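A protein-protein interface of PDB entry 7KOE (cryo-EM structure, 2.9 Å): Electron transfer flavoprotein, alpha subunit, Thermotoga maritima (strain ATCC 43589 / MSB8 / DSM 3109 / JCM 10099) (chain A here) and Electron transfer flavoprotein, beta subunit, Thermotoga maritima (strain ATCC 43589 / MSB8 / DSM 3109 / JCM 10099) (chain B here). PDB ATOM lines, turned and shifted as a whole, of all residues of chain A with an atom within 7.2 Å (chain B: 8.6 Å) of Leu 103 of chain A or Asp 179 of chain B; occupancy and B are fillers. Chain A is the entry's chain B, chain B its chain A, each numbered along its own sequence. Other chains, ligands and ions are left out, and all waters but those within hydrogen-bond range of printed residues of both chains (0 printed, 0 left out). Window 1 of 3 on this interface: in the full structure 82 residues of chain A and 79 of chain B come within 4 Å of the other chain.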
ATOM      1  N   GLU A  12      16.658 -14.422   2.971  1.00  0.00           N
ATOM      2  CA  GLU A  12      15.841 -14.107   4.137  1.00  0.00           C
ATOM      3  C   GLU A  12      16.753 -14.045   5.353  1.00  0.00           C
ATOM      4  O   GLU A  12      17.253 -15.076   5.807  1.00  0.00           O
ATOM      5  CB  GLU A  12      14.753 -15.162   4.330  1.00  0.00           C
ATOM      6  CG  GLU A  12      13.712 -15.240   3.222  1.00  0.00           C
ATOM      7  CD  GLU A  12      12.745 -14.070   3.225  1.00  0.00           C
ATOM      8  OE1 GLU A  12      12.093 -13.842   2.186  1.00  0.00           O
ATOM      9  OE2 GLU A  12      12.609 -13.399   4.270  1.00  0.00           O
ATOM     10  N   HIS A  14      17.309 -12.740   9.424  1.00  0.00           N
ATOM     11  CA  HIS A  14      16.577 -12.468  10.658  1.00  0.00           C
ATOM     12  C   HIS A  14      17.525 -11.758  11.618  1.00  0.00           C
ATOM     13  O   HIS A  14      18.207 -12.391  12.426  1.00  0.00           O
ATOM     14  CB  HIS A  14      16.022 -13.752  11.246  1.00  0.00           C
ATOM     15  CG  HIS A  14      15.103 -14.482  10.318  1.00  0.00           C
ATOM     16  ND1 HIS A  14      14.020 -13.875   9.720  1.00  0.00           N
ATOM     17  CD2 HIS A  14      15.111 -15.761   9.876  1.00  0.00           C
ATOM     18  CE1 HIS A  14      13.397 -14.750   8.952  1.00  0.00           C
ATOM     19  NE2 HIS A  14      14.038 -15.902   9.030  1.00  0.00           N
ATOM     20  N   HIS A  19      18.268 -16.956   6.947  1.00  0.00           N
ATOM     21  CA  HIS A  19      17.568 -18.223   7.005  1.00  0.00           C
ATOM     22  C   HIS A  19      18.360 -19.264   6.225  1.00  0.00           C
ATOM     23  O   HIS A  19      19.041 -18.929   5.252  1.00  0.00           O
ATOM     24  CB  HIS A  19      16.161 -18.092   6.422  1.00  0.00           C
ATOM     25  CG  HIS A  19      15.171 -19.055   7.000  1.00  0.00           C
ATOM     26  ND1 HIS A  19      15.003 -20.334   6.514  1.00  0.00           N
ATOM     27  CD2 HIS A  19      14.298 -18.928   8.027  1.00  0.00           C
ATOM     28  CE1 HIS A  19      14.071 -20.952   7.216  1.00  0.00           C
ATOM     29  NE2 HIS A  19      13.626 -20.120   8.139  1.00  0.00           N
ATOM     30  N   TYR A  76      11.338  -6.861   9.053  1.00  0.00           N
ATOM     31  CA  TYR A  76      10.538  -7.324   7.927  1.00  0.00           C
ATOM     32  C   TYR A  76       9.238  -6.535   7.883  1.00  0.00           C
ATOM     33  O   TYR A  76       8.371  -6.703   8.745  1.00  0.00           O
ATOM     34  CB  TYR A  76      10.250  -8.818   8.015  1.00  0.00           C
ATOM     35  CG  TYR A  76       9.275  -9.257   6.951  1.00  0.00           C
ATOM     36  CD1 TYR A  76       9.641  -9.251   5.614  1.00  0.00           C
ATOM     37  CD2 TYR A  76       7.983  -9.654   7.278  1.00  0.00           C
ATOM     38  CE1 TYR A  76       8.756  -9.639   4.633  1.00  0.00           C
ATOM     39  CE2 TYR A  76       7.089 -10.042   6.299  1.00  0.00           C
ATOM     40  CZ  TYR A  76       7.485 -10.031   4.980  1.00  0.00           C
ATOM     41  OH  TYR A  76       6.608 -10.420   4.000  1.00  0.00           O
ATOM     42  N   GLY A 100      12.293 -18.348  -0.577  1.00  0.00           N
ATOM     43  CA  GLY A 100      11.905 -19.493   0.216  1.00  0.00           C
ATOM     44  C   GLY A 100      10.469 -19.391   0.690  1.00  0.00           C
ATOM     45  O   GLY A 100       9.900 -18.306   0.805  1.00  0.00           O
ATOM     46  N   ALA A 101       9.865 -20.541   0.973  1.00  0.00           N
ATOM     47  CA  ALA A 101       8.481 -20.550   1.453  1.00  0.00           C
ATOM     48  C   ALA A 101       8.407 -20.464   2.967  1.00  0.00           C
ATOM     49  O   ALA A 101       7.764 -21.266   3.639  1.00  0.00           O
ATOM     50  CB  ALA A 101       7.736 -21.775   0.940  1.00  0.00           C
ATOM     51  N   THR A 102       9.086 -19.465   3.512  1.00  0.00           N
ATOM     52  CA  THR A 102       8.803 -19.022   4.857  1.00  0.00           C
ATOM     53  C   THR A 102       7.525 -18.190   4.842  1.00  0.00           C
ATOM     54  O   THR A 102       7.002 -17.834   3.784  1.00  0.00           O
ATOM     55  CB  THR A 102       9.983 -18.224   5.406  1.00  0.00           C
ATOM     56  OG1 THR A 102       9.988 -16.914   4.829  1.00  0.00           O
ATOM     57  CG2 THR A 102      11.287 -18.916   5.072  1.00  0.00           C
ATOM     58  N   LEU A 103       7.007 -17.886   6.034  1.00  0.00           N
ATOM     59  CA  LEU A 103       5.774 -17.111   6.102  1.00  0.00           C
ATOM     60  C   LEU A 103       5.987 -15.672   5.649  1.00  0.00           C
ATOM     61  O   LEU A 103       5.067 -15.055   5.107  1.00  0.00           O
ATOM     62  CB  LEU A 103       5.195 -17.154   7.514  1.00  0.00           C
ATOM     63  CG  LEU A 103       4.603 -18.493   7.961  1.00  0.00           C
ATOM     64  CD1 LEU A 103       3.871 -18.336   9.274  1.00  0.00           C
ATOM     65  CD2 LEU A 103       3.674 -19.057   6.907  1.00  0.00           C
ATOM     66  N   GLU A 104       7.190 -15.130   5.830  1.00  0.00           N
ATOM     67  CA  GLU A 104       7.496 -13.857   5.191  1.00  0.00           C
ATOM     68  C   GLU A 104       7.705 -14.014   3.694  1.00  0.00           C
ATOM     69  O   GLU A 104       7.379 -13.101   2.937  1.00  0.00           O
ATOM     70  CB  GLU A 104       8.735 -13.216   5.815  1.00  0.00           C
ATOM     71  CG  GLU A 104       8.795 -13.274   7.325  1.00  0.00           C
ATOM     72  CD  GLU A 104       9.648 -14.410   7.830  1.00  0.00           C
ATOM     73  OE1 GLU A 104       9.687 -15.466   7.174  1.00  0.00           O
ATOM     74  OE2 GLU A 104      10.300 -14.238   8.874  1.00  0.00           O
ATOM     75  N   GLY A 105       8.227 -15.152   3.252  1.00  0.00           N
ATOM     76  CA  GLY A 105       8.524 -15.351   1.849  1.00  0.00           C
ATOM     77  C   GLY A 105       7.300 -15.541   0.981  1.00  0.00           C
ATOM     78  O   GLY A 105       7.232 -15.000  -0.125  1.00  0.00           O
ATOM     79  N   ARG A 106       6.327 -16.315   1.469  1.00  0.00           N
ATOM     80  CA  ARG A 106       5.086 -16.504   0.726  1.00  0.00           C
ATOM     81  C   ARG A 106       4.247 -15.236   0.702  1.00  0.00           C
ATOM     82  O   ARG A 106       3.542 -14.979  -0.278  1.00  0.00           O
ATOM     83  CB  ARG A 106       4.278 -17.648   1.329  1.00  0.00           C
ATOM     84  CG  ARG A 106       5.006 -18.968   1.364  1.00  0.00           C
ATOM     85  CD  ARG A 106       4.088 -20.085   1.809  1.00  0.00           C
ATOM     86  NE  ARG A 106       3.026 -20.328   0.842  1.00  0.00           N
ATOM     87  CZ  ARG A 106       2.466 -21.514   0.636  1.00  0.00           C
ATOM     88  NH1 ARG A 106       2.868 -22.566   1.332  1.00  0.00           N
ATOM     89  NH2 ARG A 106       1.507 -21.648  -0.266  1.00  0.00           N
ATOM     90  N   GLU A 107       4.305 -14.441   1.768  1.00  0.00           N
ATOM     91  CA  GLU A 107       3.559 -13.191   1.803  1.00  0.00           C
ATOM     92  C   GLU A 107       4.201 -12.145   0.901  1.00  0.00           C
ATOM     93  O   GLU A 107       3.498 -11.385   0.225  1.00  0.00           O
ATOM     94  CB  GLU A 107       3.461 -12.704   3.250  1.00  0.00           C
ATOM     95  CG  GLU A 107       3.387 -11.208   3.441  1.00  0.00           C
ATOM     96  CD  GLU A 107       3.132 -10.825   4.876  1.00  0.00           C
ATOM     97  OE1 GLU A 107       3.512 -11.598   5.776  1.00  0.00           O
ATOM     98  OE2 GLU A 107       2.541  -9.755   5.106  1.00  0.00           O
ATOM     99  N   LEU A 108       5.534 -12.122   0.847  1.00  0.00           N
ATOM    100  CA  LEU A 108       6.244 -11.144   0.029  1.00  0.00           C
ATOM    101  C   LEU A 108       6.096 -11.441  -1.454  1.00  0.00           C
ATOM    102  O   LEU A 108       5.940 -10.518  -2.260  1.00  0.00           O
ATOM    103  CB  LEU A 108       7.720 -11.132   0.407  1.00  0.00           C
ATOM    104  CG  LEU A 108       8.652  -9.978   0.068  1.00  0.00           C
ATOM    105  CD1 LEU A 108       9.678  -9.935   1.153  1.00  0.00           C
ATOM    106  CD2 LEU A 108       9.334 -10.199  -1.258  1.00  0.00           C
ATOM    107  N   PRO A 165      11.092 -24.649   2.129  1.00  0.00           N
ATOM    108  CA  PRO A 165      12.384 -24.793   2.813  1.00  0.00           C
ATOM    109  C   PRO A 165      12.653 -26.239   3.200  1.00  0.00           C
ATOM    110  O   PRO A 165      11.895 -26.844   3.963  1.00  0.00           O
ATOM    111  CB  PRO A 165      12.230 -23.898   4.048  1.00  0.00           C
ATOM    112  CG  PRO A 165      11.091 -22.989   3.729  1.00  0.00           C
ATOM    113  CD  PRO A 165      10.165 -23.812   2.902  1.00  0.00           C
ATOM    114  N   LEU A 203       7.257 -17.881  19.571  1.00  0.00           N
ATOM    115  CA  LEU A 203       6.439 -18.873  18.888  1.00  0.00           C
ATOM    116  C   LEU A 203       5.930 -19.966  19.814  1.00  0.00           C
ATOM    117  O   LEU A 203       4.929 -20.612  19.490  1.00  0.00           O
ATOM    118  CB  LEU A 203       7.238 -19.498  17.742  1.00  0.00           C
ATOM    119  CG  LEU A 203       6.472 -20.102  16.565  1.00  0.00           C
ATOM    120  CD1 LEU A 203       5.605 -19.064  15.881  1.00  0.00           C
ATOM    121  CD2 LEU A 203       7.438 -20.730  15.576  1.00  0.00           C
ATOM    122  N   TYR A 211       4.027 -25.276  11.881  1.00  0.00           N
ATOM    123  CA  TYR A 211       5.275 -24.576  11.631  1.00  0.00           C
ATOM    124  C   TYR A 211       6.327 -24.976  12.651  1.00  0.00           C
ATOM    125  O   TYR A 211       7.267 -24.219  12.909  1.00  0.00           O
ATOM    126  CB  TYR A 211       5.036 -23.066  11.639  1.00  0.00           C
ATOM    127  CG  TYR A 211       3.815 -22.664  10.841  1.00  0.00           C
ATOM    128  CD1 TYR A 211       3.884 -22.505   9.463  1.00  0.00           C
ATOM    129  CD2 TYR A 211       2.588 -22.454  11.462  1.00  0.00           C
ATOM    130  CE1 TYR A 211       2.770 -22.145   8.730  1.00  0.00           C
ATOM    131  CE2 TYR A 211       1.473 -22.106  10.737  1.00  0.00           C
ATOM    132  CZ  TYR A 211       1.572 -21.945   9.376  1.00  0.00           C
ATOM    133  OH  TYR A 211       0.458 -21.588   8.660  1.00  0.00           O
ATOM    134  N   LYS B 133      -6.073 -17.839   4.827  1.00  0.00           N
ATOM    135  CA  LYS B 133      -4.634 -18.032   4.706  1.00  0.00           C
ATOM    136  C   LYS B 133      -4.298 -18.826   3.454  1.00  0.00           C
ATOM    137  O   LYS B 133      -3.333 -18.516   2.747  1.00  0.00           O
ATOM    138  CB  LYS B 133      -4.097 -18.721   5.959  1.00  0.00           C
ATOM    139  CG  LYS B 133      -2.598 -18.860   5.997  1.00  0.00           C
ATOM    140  CD  LYS B 133      -2.178 -20.314   5.918  1.00  0.00           C
ATOM    141  CE  LYS B 133      -0.674 -20.437   5.808  1.00  0.00           C
ATOM    142  NZ  LYS B 133      -0.223 -21.852   5.735  1.00  0.00           N
ATOM    143  N   GLN B 134      -5.108 -19.829   3.144  1.00  0.00           N
ATOM    144  CA  GLN B 134      -4.891 -20.677   1.988  1.00  0.00           C
ATOM    145  C   GLN B 134      -6.217 -21.281   1.569  1.00  0.00           C
ATOM    146  O   GLN B 134      -7.063 -21.588   2.407  1.00  0.00           O
ATOM    147  CB  GLN B 134      -3.911 -21.810   2.295  1.00  0.00           C
ATOM    148  CG  GLN B 134      -2.479 -21.564   1.920  1.00  0.00           C
ATOM    149  CD  GLN B 134      -1.614 -22.748   2.259  1.00  0.00           C
ATOM    150  OE1 GLN B 134      -2.115 -23.788   2.677  1.00  0.00           O
ATOM    151  NE2 GLN B 134      -0.310 -22.600   2.088  1.00  0.00           N
ATOM    152  N   GLY B 141      -2.034 -19.468  -1.505  1.00  0.00           N
ATOM    153  CA  GLY B 141      -2.150 -18.422  -0.515  1.00  0.00           C
ATOM    154  C   GLY B 141      -1.676 -17.072  -0.985  1.00  0.00           C
ATOM    155  O   GLY B 141      -1.304 -16.237  -0.160  1.00  0.00           O
ATOM    156  N   PRO B 145      -2.307 -11.792  -0.309  1.00  0.00           N
ATOM    157  CA  PRO B 145      -1.208 -10.869  -0.630  1.00  0.00           C
ATOM    158  C   PRO B 145      -1.376 -10.123  -1.941  1.00  0.00           C
ATOM    159  O   PRO B 145      -1.010  -8.945  -2.020  1.00  0.00           O
ATOM    160  CB  PRO B 145       0.006 -11.799  -0.667  1.00  0.00           C
ATOM    161  CG  PRO B 145      -0.306 -12.824   0.328  1.00  0.00           C
ATOM    162  CD  PRO B 145      -1.792 -13.026   0.311  1.00  0.00           C
ATOM    163  N   LEU B 155      -1.255  -5.013   4.073  1.00  0.00           N
ATOM    164  CA  LEU B 155      -1.415  -6.460   4.129  1.00  0.00           C
ATOM    165  C   LEU B 155      -1.057  -6.949   5.523  1.00  0.00           C
ATOM    166  O   LEU B 155       0.118  -6.961   5.901  1.00  0.00           O
ATOM    167  CB  LEU B 155      -0.542  -7.152   3.091  1.00  0.00           C
ATOM    168  CG  LEU B 155      -0.639  -8.672   3.160  1.00  0.00           C
ATOM    169  CD1 LEU B 155      -2.010  -9.136   2.725  1.00  0.00           C
ATOM    170  CD2 LEU B 155       0.427  -9.300   2.314  1.00  0.00           C
ATOM    171  N   ALA B 157      -1.096 -10.369   6.997  1.00  0.00           N
ATOM    172  CA  ALA B 157      -1.306 -11.767   6.670  1.00  0.00           C
ATOM    173  C   ALA B 157      -1.042 -12.640   7.885  1.00  0.00           C
ATOM    174  O   ALA B 157      -0.365 -12.229   8.826  1.00  0.00           O
ATOM    175  CB  ALA B 157      -0.415 -12.187   5.501  1.00  0.00           C
ATOM    176  N   TYR B 158      -1.610 -13.853   7.847  1.00  0.00           N
ATOM    177  CA  TYR B 158      -1.476 -14.878   8.892  1.00  0.00           C
ATOM    178  C   TYR B 158      -1.946 -14.375  10.255  1.00  0.00           C
ATOM    179  O   TYR B 158      -1.247 -14.494  11.260  1.00  0.00           O
ATOM    180  CB  TYR B 158      -0.045 -15.413   8.970  1.00  0.00           C
ATOM    181  CG  TYR B 158       0.552 -15.712   7.625  1.00  0.00           C
ATOM    182  CD1 TYR B 158       0.223 -16.870   6.946  1.00  0.00           C
ATOM    183  CD2 TYR B 158       1.446 -14.836   7.032  1.00  0.00           C
ATOM    184  CE1 TYR B 158       0.760 -17.147   5.712  1.00  0.00           C
ATOM    185  CE2 TYR B 158       1.981 -15.099   5.796  1.00  0.00           C
ATOM    186  CZ  TYR B 158       1.640 -16.260   5.143  1.00  0.00           C
ATOM    187  OH  TYR B 158       2.176 -16.539   3.910  1.00  0.00           O
ATOM    188  N   VAL B 159      -3.152 -13.826  10.285  1.00  0.00           N
ATOM    189  CA  VAL B 159      -3.695 -13.227  11.498  1.00  0.00           C
ATOM    190  C   VAL B 159      -4.117 -14.323  12.463  1.00  0.00           C
ATOM    191  O   VAL B 159      -4.868 -15.233  12.099  1.00  0.00           O
ATOM    192  CB  VAL B 159      -4.872 -12.309  11.159  1.00  0.00           C
ATOM    193  CG1 VAL B 159      -5.354 -11.600  12.390  1.00  0.00           C
ATOM    194  CG2 VAL B 159      -4.457 -11.331  10.113  1.00  0.00           C
ATOM    195  N   VAL B 160      -3.625 -14.242  13.699  1.00  0.00           N
ATOM    196  CA  VAL B 160      -4.015 -15.166  14.748  1.00  0.00           C
ATOM    197  C   VAL B 160      -4.906 -14.504  15.797  1.00  0.00           C
ATOM    198  O   VAL B 160      -5.795 -15.165  16.344  1.00  0.00           O
ATOM    199  CB  VAL B 160      -2.765 -15.796  15.400  1.00  0.00           C
ATOM    200  CG1 VAL B 160      -3.126 -16.961  16.304  1.00  0.00           C
ATOM    201  CG2 VAL B 160      -1.834 -16.279  14.335  1.00  0.00           C
ATOM    202  N   ARG B 176       0.051 -11.053  13.679  1.00  0.00           N
ATOM    203  CA  ARG B 176       0.470 -11.872  12.552  1.00  0.00           C
ATOM    204  C   ARG B 176       1.435 -12.950  13.021  1.00  0.00           C
ATOM    205  O   ARG B 176       2.341 -12.684  13.810  1.00  0.00           O
ATOM    206  CB  ARG B 176       1.129 -10.993  11.485  1.00  0.00           C
ATOM    207  CG  ARG B 176       2.244 -11.661  10.684  1.00  0.00           C
ATOM    208  CD  ARG B 176       3.125 -10.666   9.977  1.00  0.00           C
ATOM    209  NE  ARG B 176       2.456 -10.034   8.851  1.00  0.00           N
ATOM    210  CZ  ARG B 176       2.959  -9.007   8.178  1.00  0.00           C
ATOM    211  NH1 ARG B 176       4.133  -8.501   8.525  1.00  0.00           N
ATOM    212  NH2 ARG B 176       2.289  -8.482   7.162  1.00  0.00           N
ATOM    213  N   ARG B 177       1.235 -14.173  12.545  1.00  0.00           N
ATOM    214  CA  ARG B 177       2.179 -15.251  12.798  1.00  0.00           C
ATOM    215  C   ARG B 177       3.271 -15.248  11.739  1.00  0.00           C
ATOM    216  O   ARG B 177       2.981 -15.230  10.541  1.00  0.00           O
ATOM    217  CB  ARG B 177       1.472 -16.603  12.800  1.00  0.00           C
ATOM    218  CG  ARG B 177       2.405 -17.789  12.758  1.00  0.00           C
ATOM    219  CD  ARG B 177       1.638 -19.064  12.562  1.00  0.00           C
ATOM    220  NE  ARG B 177       1.000 -19.508  13.793  1.00  0.00           N
ATOM    221  CZ  ARG B 177       1.547 -20.368  14.643  1.00  0.00           C
ATOM    222  NH1 ARG B 177       2.747 -20.869  14.397  1.00  0.00           N
ATOM    223  NH2 ARG B 177       0.896 -20.720  15.742  1.00  0.00           N
ATOM    224  N   LEU B 178       4.519 -15.265  12.184  1.00  0.00           N
ATOM    225  CA  LEU B 178       5.667 -15.500  11.324  1.00  0.00           C
ATOM    226  C   LEU B 178       6.412 -16.729  11.833  1.00  0.00           C
ATOM    227  O   LEU B 178       5.966 -17.412  12.755  1.00  0.00           O
ATOM    228  CB  LEU B 178       6.572 -14.269  11.271  1.00  0.00           C
ATOM    229  CG  LEU B 178       5.966 -13.077  10.534  1.00  0.00           C
ATOM    230  CD1 LEU B 178       6.952 -11.935  10.463  1.00  0.00           C
ATOM    231  CD2 LEU B 178       5.512 -13.476   9.141  1.00  0.00           C
ATOM    232  N   ASP B 179       7.560 -17.016  11.223  1.00  0.00           N
ATOM    233  CA  ASP B 179       8.296 -18.213  11.608  1.00  0.00           C
ATOM    234  C   ASP B 179       9.194 -17.985  12.816  1.00  0.00           C
ATOM    235  O   ASP B 179       9.458 -18.929  13.568  1.00  0.00           O
ATOM    236  CB  ASP B 179       9.114 -18.730  10.431  1.00  0.00           C
ATOM    237  CG  ASP B 179       8.251 -19.377   9.376  1.00  0.00           C
ATOM    238  OD1 ASP B 179       7.177 -19.908   9.730  1.00  0.00           O
ATOM    239  OD2 ASP B 179       8.646 -19.367   8.198  1.00  0.00           O
ATOM    240  N   GLN B 180       9.676 -16.761  13.022  1.00  0.00           N
ATOM    241  CA  GLN B 180      10.414 -16.466  14.241  1.00  0.00           C
ATOM    242  C   GLN B 180       9.495 -16.207  15.422  1.00  0.00           C
ATOM    243  O   GLN B 180       9.969 -16.178  16.562  1.00  0.00           O
ATOM    244  CB  GLN B 180      11.330 -15.257  14.033  1.00  0.00           C
ATOM    245  CG  GLN B 180      10.615 -13.915  13.977  1.00  0.00           C
ATOM    246  CD  GLN B 180      10.140 -13.552  12.587  1.00  0.00           C
ATOM    247  OE1 GLN B 180      10.046 -14.405  11.710  1.00  0.00           O
ATOM    248  NE2 GLN B 180       9.844 -12.277  12.378  1.00  0.00           N
ATOM    249  N   GLY B 181       8.202 -16.026  15.180  1.00  0.00           N
ATOM    250  CA  GLY B 181       7.261 -15.766  16.245  1.00  0.00           C
ATOM    251  C   GLY B 181       6.146 -14.843  15.811  1.00  0.00           C
ATOM    252  O   GLY B 181       6.174 -14.294  14.709  1.00  0.00           O
ATOM    253  N   PHE B 182       5.155 -14.672  16.674  1.00  0.00           N
ATOM    254  CA  PHE B 182       4.064 -13.758  16.395  1.00  0.00           C
ATOM    255  C   PHE B 182       4.526 -12.318  16.566  1.00  0.00           C
ATOM    256  O   PHE B 182       5.551 -12.044  17.188  1.00  0.00           O
ATOM    257  CB  PHE B 182       2.888 -14.042  17.320  1.00  0.00           C
ATOM    258  CG  PHE B 182       2.561 -15.491  17.443  1.00  0.00           C
ATOM    259  CD1 PHE B 182       1.918 -16.152  16.417  1.00  0.00           C
ATOM    260  CD2 PHE B 182       2.903 -16.194  18.582  1.00  0.00           C
ATOM    261  CE1 PHE B 182       1.617 -17.488  16.525  1.00  0.00           C
ATOM    262  CE2 PHE B 182       2.605 -17.532  18.697  1.00  0.00           C
ATOM    263  CZ  PHE B 182       1.961 -18.180  17.666  1.00  0.00           C
ATOM    264  N   GLU B 183       3.754 -11.391  16.007  1.00  0.00           N
ATOM    265  CA  GLU B 183       4.058  -9.978  16.179  1.00  0.00           C
ATOM    266  C   GLU B 183       2.781  -9.159  16.105  1.00  0.00           C
ATOM    267  O   GLU B 183       1.967  -9.356  15.201  1.00  0.00           O
ATOM    268  CB  GLU B 183       5.057  -9.493  15.126  1.00  0.00           C
ATOM    269  CG  GLU B 183       4.809  -9.995  13.726  1.00  0.00           C
ATOM    270  CD  GLU B 183       5.826  -9.457  12.747  1.00  0.00           C
ATOM    271  OE1 GLU B 183       7.032  -9.499  13.064  1.00  0.00           O
ATOM    272  OE2 GLU B 183       5.427  -8.981  11.665  1.00  0.00           O
ATOM    273  N   THR B 196      -6.049 -17.106   9.506  1.00  0.00           N
ATOM    274  CA  THR B 196      -5.707 -18.505   9.694  1.00  0.00           C
ATOM    275  C   THR B 196      -6.852 -19.256  10.367  1.00  0.00           C
ATOM    276  O   THR B 196      -7.929 -18.714  10.611  1.00  0.00           O
ATOM    277  CB  THR B 196      -4.438 -18.637  10.527  1.00  0.00           C
ATOM    278  OG1 THR B 196      -4.637 -18.007  11.796  1.00  0.00           O
ATOM    279  CG2 THR B 196      -3.276 -17.993   9.825  1.00  0.00           C
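NZ of Lys 133 of chain B sits at hydrogen-bond distance from OH of Tyr 211 of chain A, 3.0 Å away.
The side-chain carboxylate (OD2) of Asp 179 of chain B lies within hydrogen-bond range of the backbone NH (N) of Leu 103 of chain A, 3.1 Å away.
The guanidinium group (NH2) of Arg 176 of chain B is in salt-bridge range of the side-chain carboxylate (OE2) of Glu 107 of chain A (2.4 Å).
The guanidinium group (NH2) of Arg 106 of chain A sits close to the side-chain amide nitrogen (NE2) of Gln 134 of chain B, 3.1 Å away.
The side-chain carboxylate (OE2) of Glu 104 of chain A lies close to the side-chain amide oxygen (OE1) of Gln 180 of chain B (2.9 Å).
The side-chain hydroxyl of Tyr 158 of chain B sits close to the backbone carbonyl oxygen of Leu 103 of chain A.
OH of Tyr 76 of chain A lies within hydrogen-bond range of O of Glu 104 of chain A, at 3.0 Å.
NH1 of Arg 176 of chain B lies within salt-bridge range of OE2 of Glu 183 of chain B.
N of Gly 105 of chain A sits at hydrogen-bond distance from OG1 of Thr 102 of chain A (2.9 Å).
The backbone carbonyl oxygen of Leu 155 of chain B is in hydrogen-bond range of the guanidinium group of Arg 176 of chain B (2.9 Å).
The side-chain hydroxyl of Thr 102 of chain A is in hydrogen-bond range of the side-chain carboxylate of Glu 104 of chain A, at 2.8 Å.
N of Arg 177 of chain B sits at hydrogen-bond distance from O of Tyr 158 of chain B, 2.8 Å away.
Among the printed residues, merely in contact across the chains: Thr 102 of chain A with Asp 179 of chain B, Tyr 211 of chain A with Arg 177 of chain B, Leu 203 of chain A with Asp 179 of chain B, Leu 103 of chain A with Arg 177 of chain B, Arg 106 of chain A with Tyr 158 of chain B, Glu 107 of chain A with Leu 155 of chain B, Leu 203 of chain A with Leu 178 of chain B, Glu 107 of chain A with Pro 145 of chain B, Glu 107 of chain A with Tyr 158 of chain B, Leu 203 of chain A with Arg 177 of chain B, Leu 203 of chain A with Gly 181 of chain B, Glu 104 of chain A with Leu 178 of chain B, Glu 107 of chain A with Ala 157 of chain B, Leu 103 of chain A with Leu 178 of chain B and Leu 203 of chain A with Phe 182 of chain B.
Leu 103 of chain A touches just these residues of chain B: Tyr 158, Arg 177, Leu 178 and Asp 179.
Of chain A, only Thr 102 (3.3 Å), Leu 103 (3.1 Å) and Leu 203 (3.4 Å) come within 4 Å of Asp 179 of chain B.
Printed residues of chain A within 4 Å of Ala 157 of chain B: Glu 107 (3.8 Å).
Of the printed residues of chain A, Phe 182 of chain B touches Leu 203 (3.9 Å).
The nearest residue of chain A that does not touch Asp 179 of chain B is Glu 104 of chain A (4.2 Å).
Hydrophobic or aromatic side chains of chain B that line the printed part of chain A: Pro 145, Leu 155, Ala 157, Tyr 158, Leu 178 and Phe 182.
Of the 16 printed residues of chain A, 7 touch a printed residue of chain B.
Printed residues of chain A that touch a printed residue of chain B: Thr 102, Leu 103, Glu 104, Arg 106, Glu 107, Leu 203 and Tyr 211.
Hydrophobic or aromatic side chains of chain A that line the printed part of chain B: Leu 103, Leu 203 and Tyr 211.
Among the printed residues, Asp or Glu carboxylates within 4 Å of a Lys or Arg side-chain nitrogen of the other chain: Glu 107 of chain A with Arg 176 of chain B (2.4 Å).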
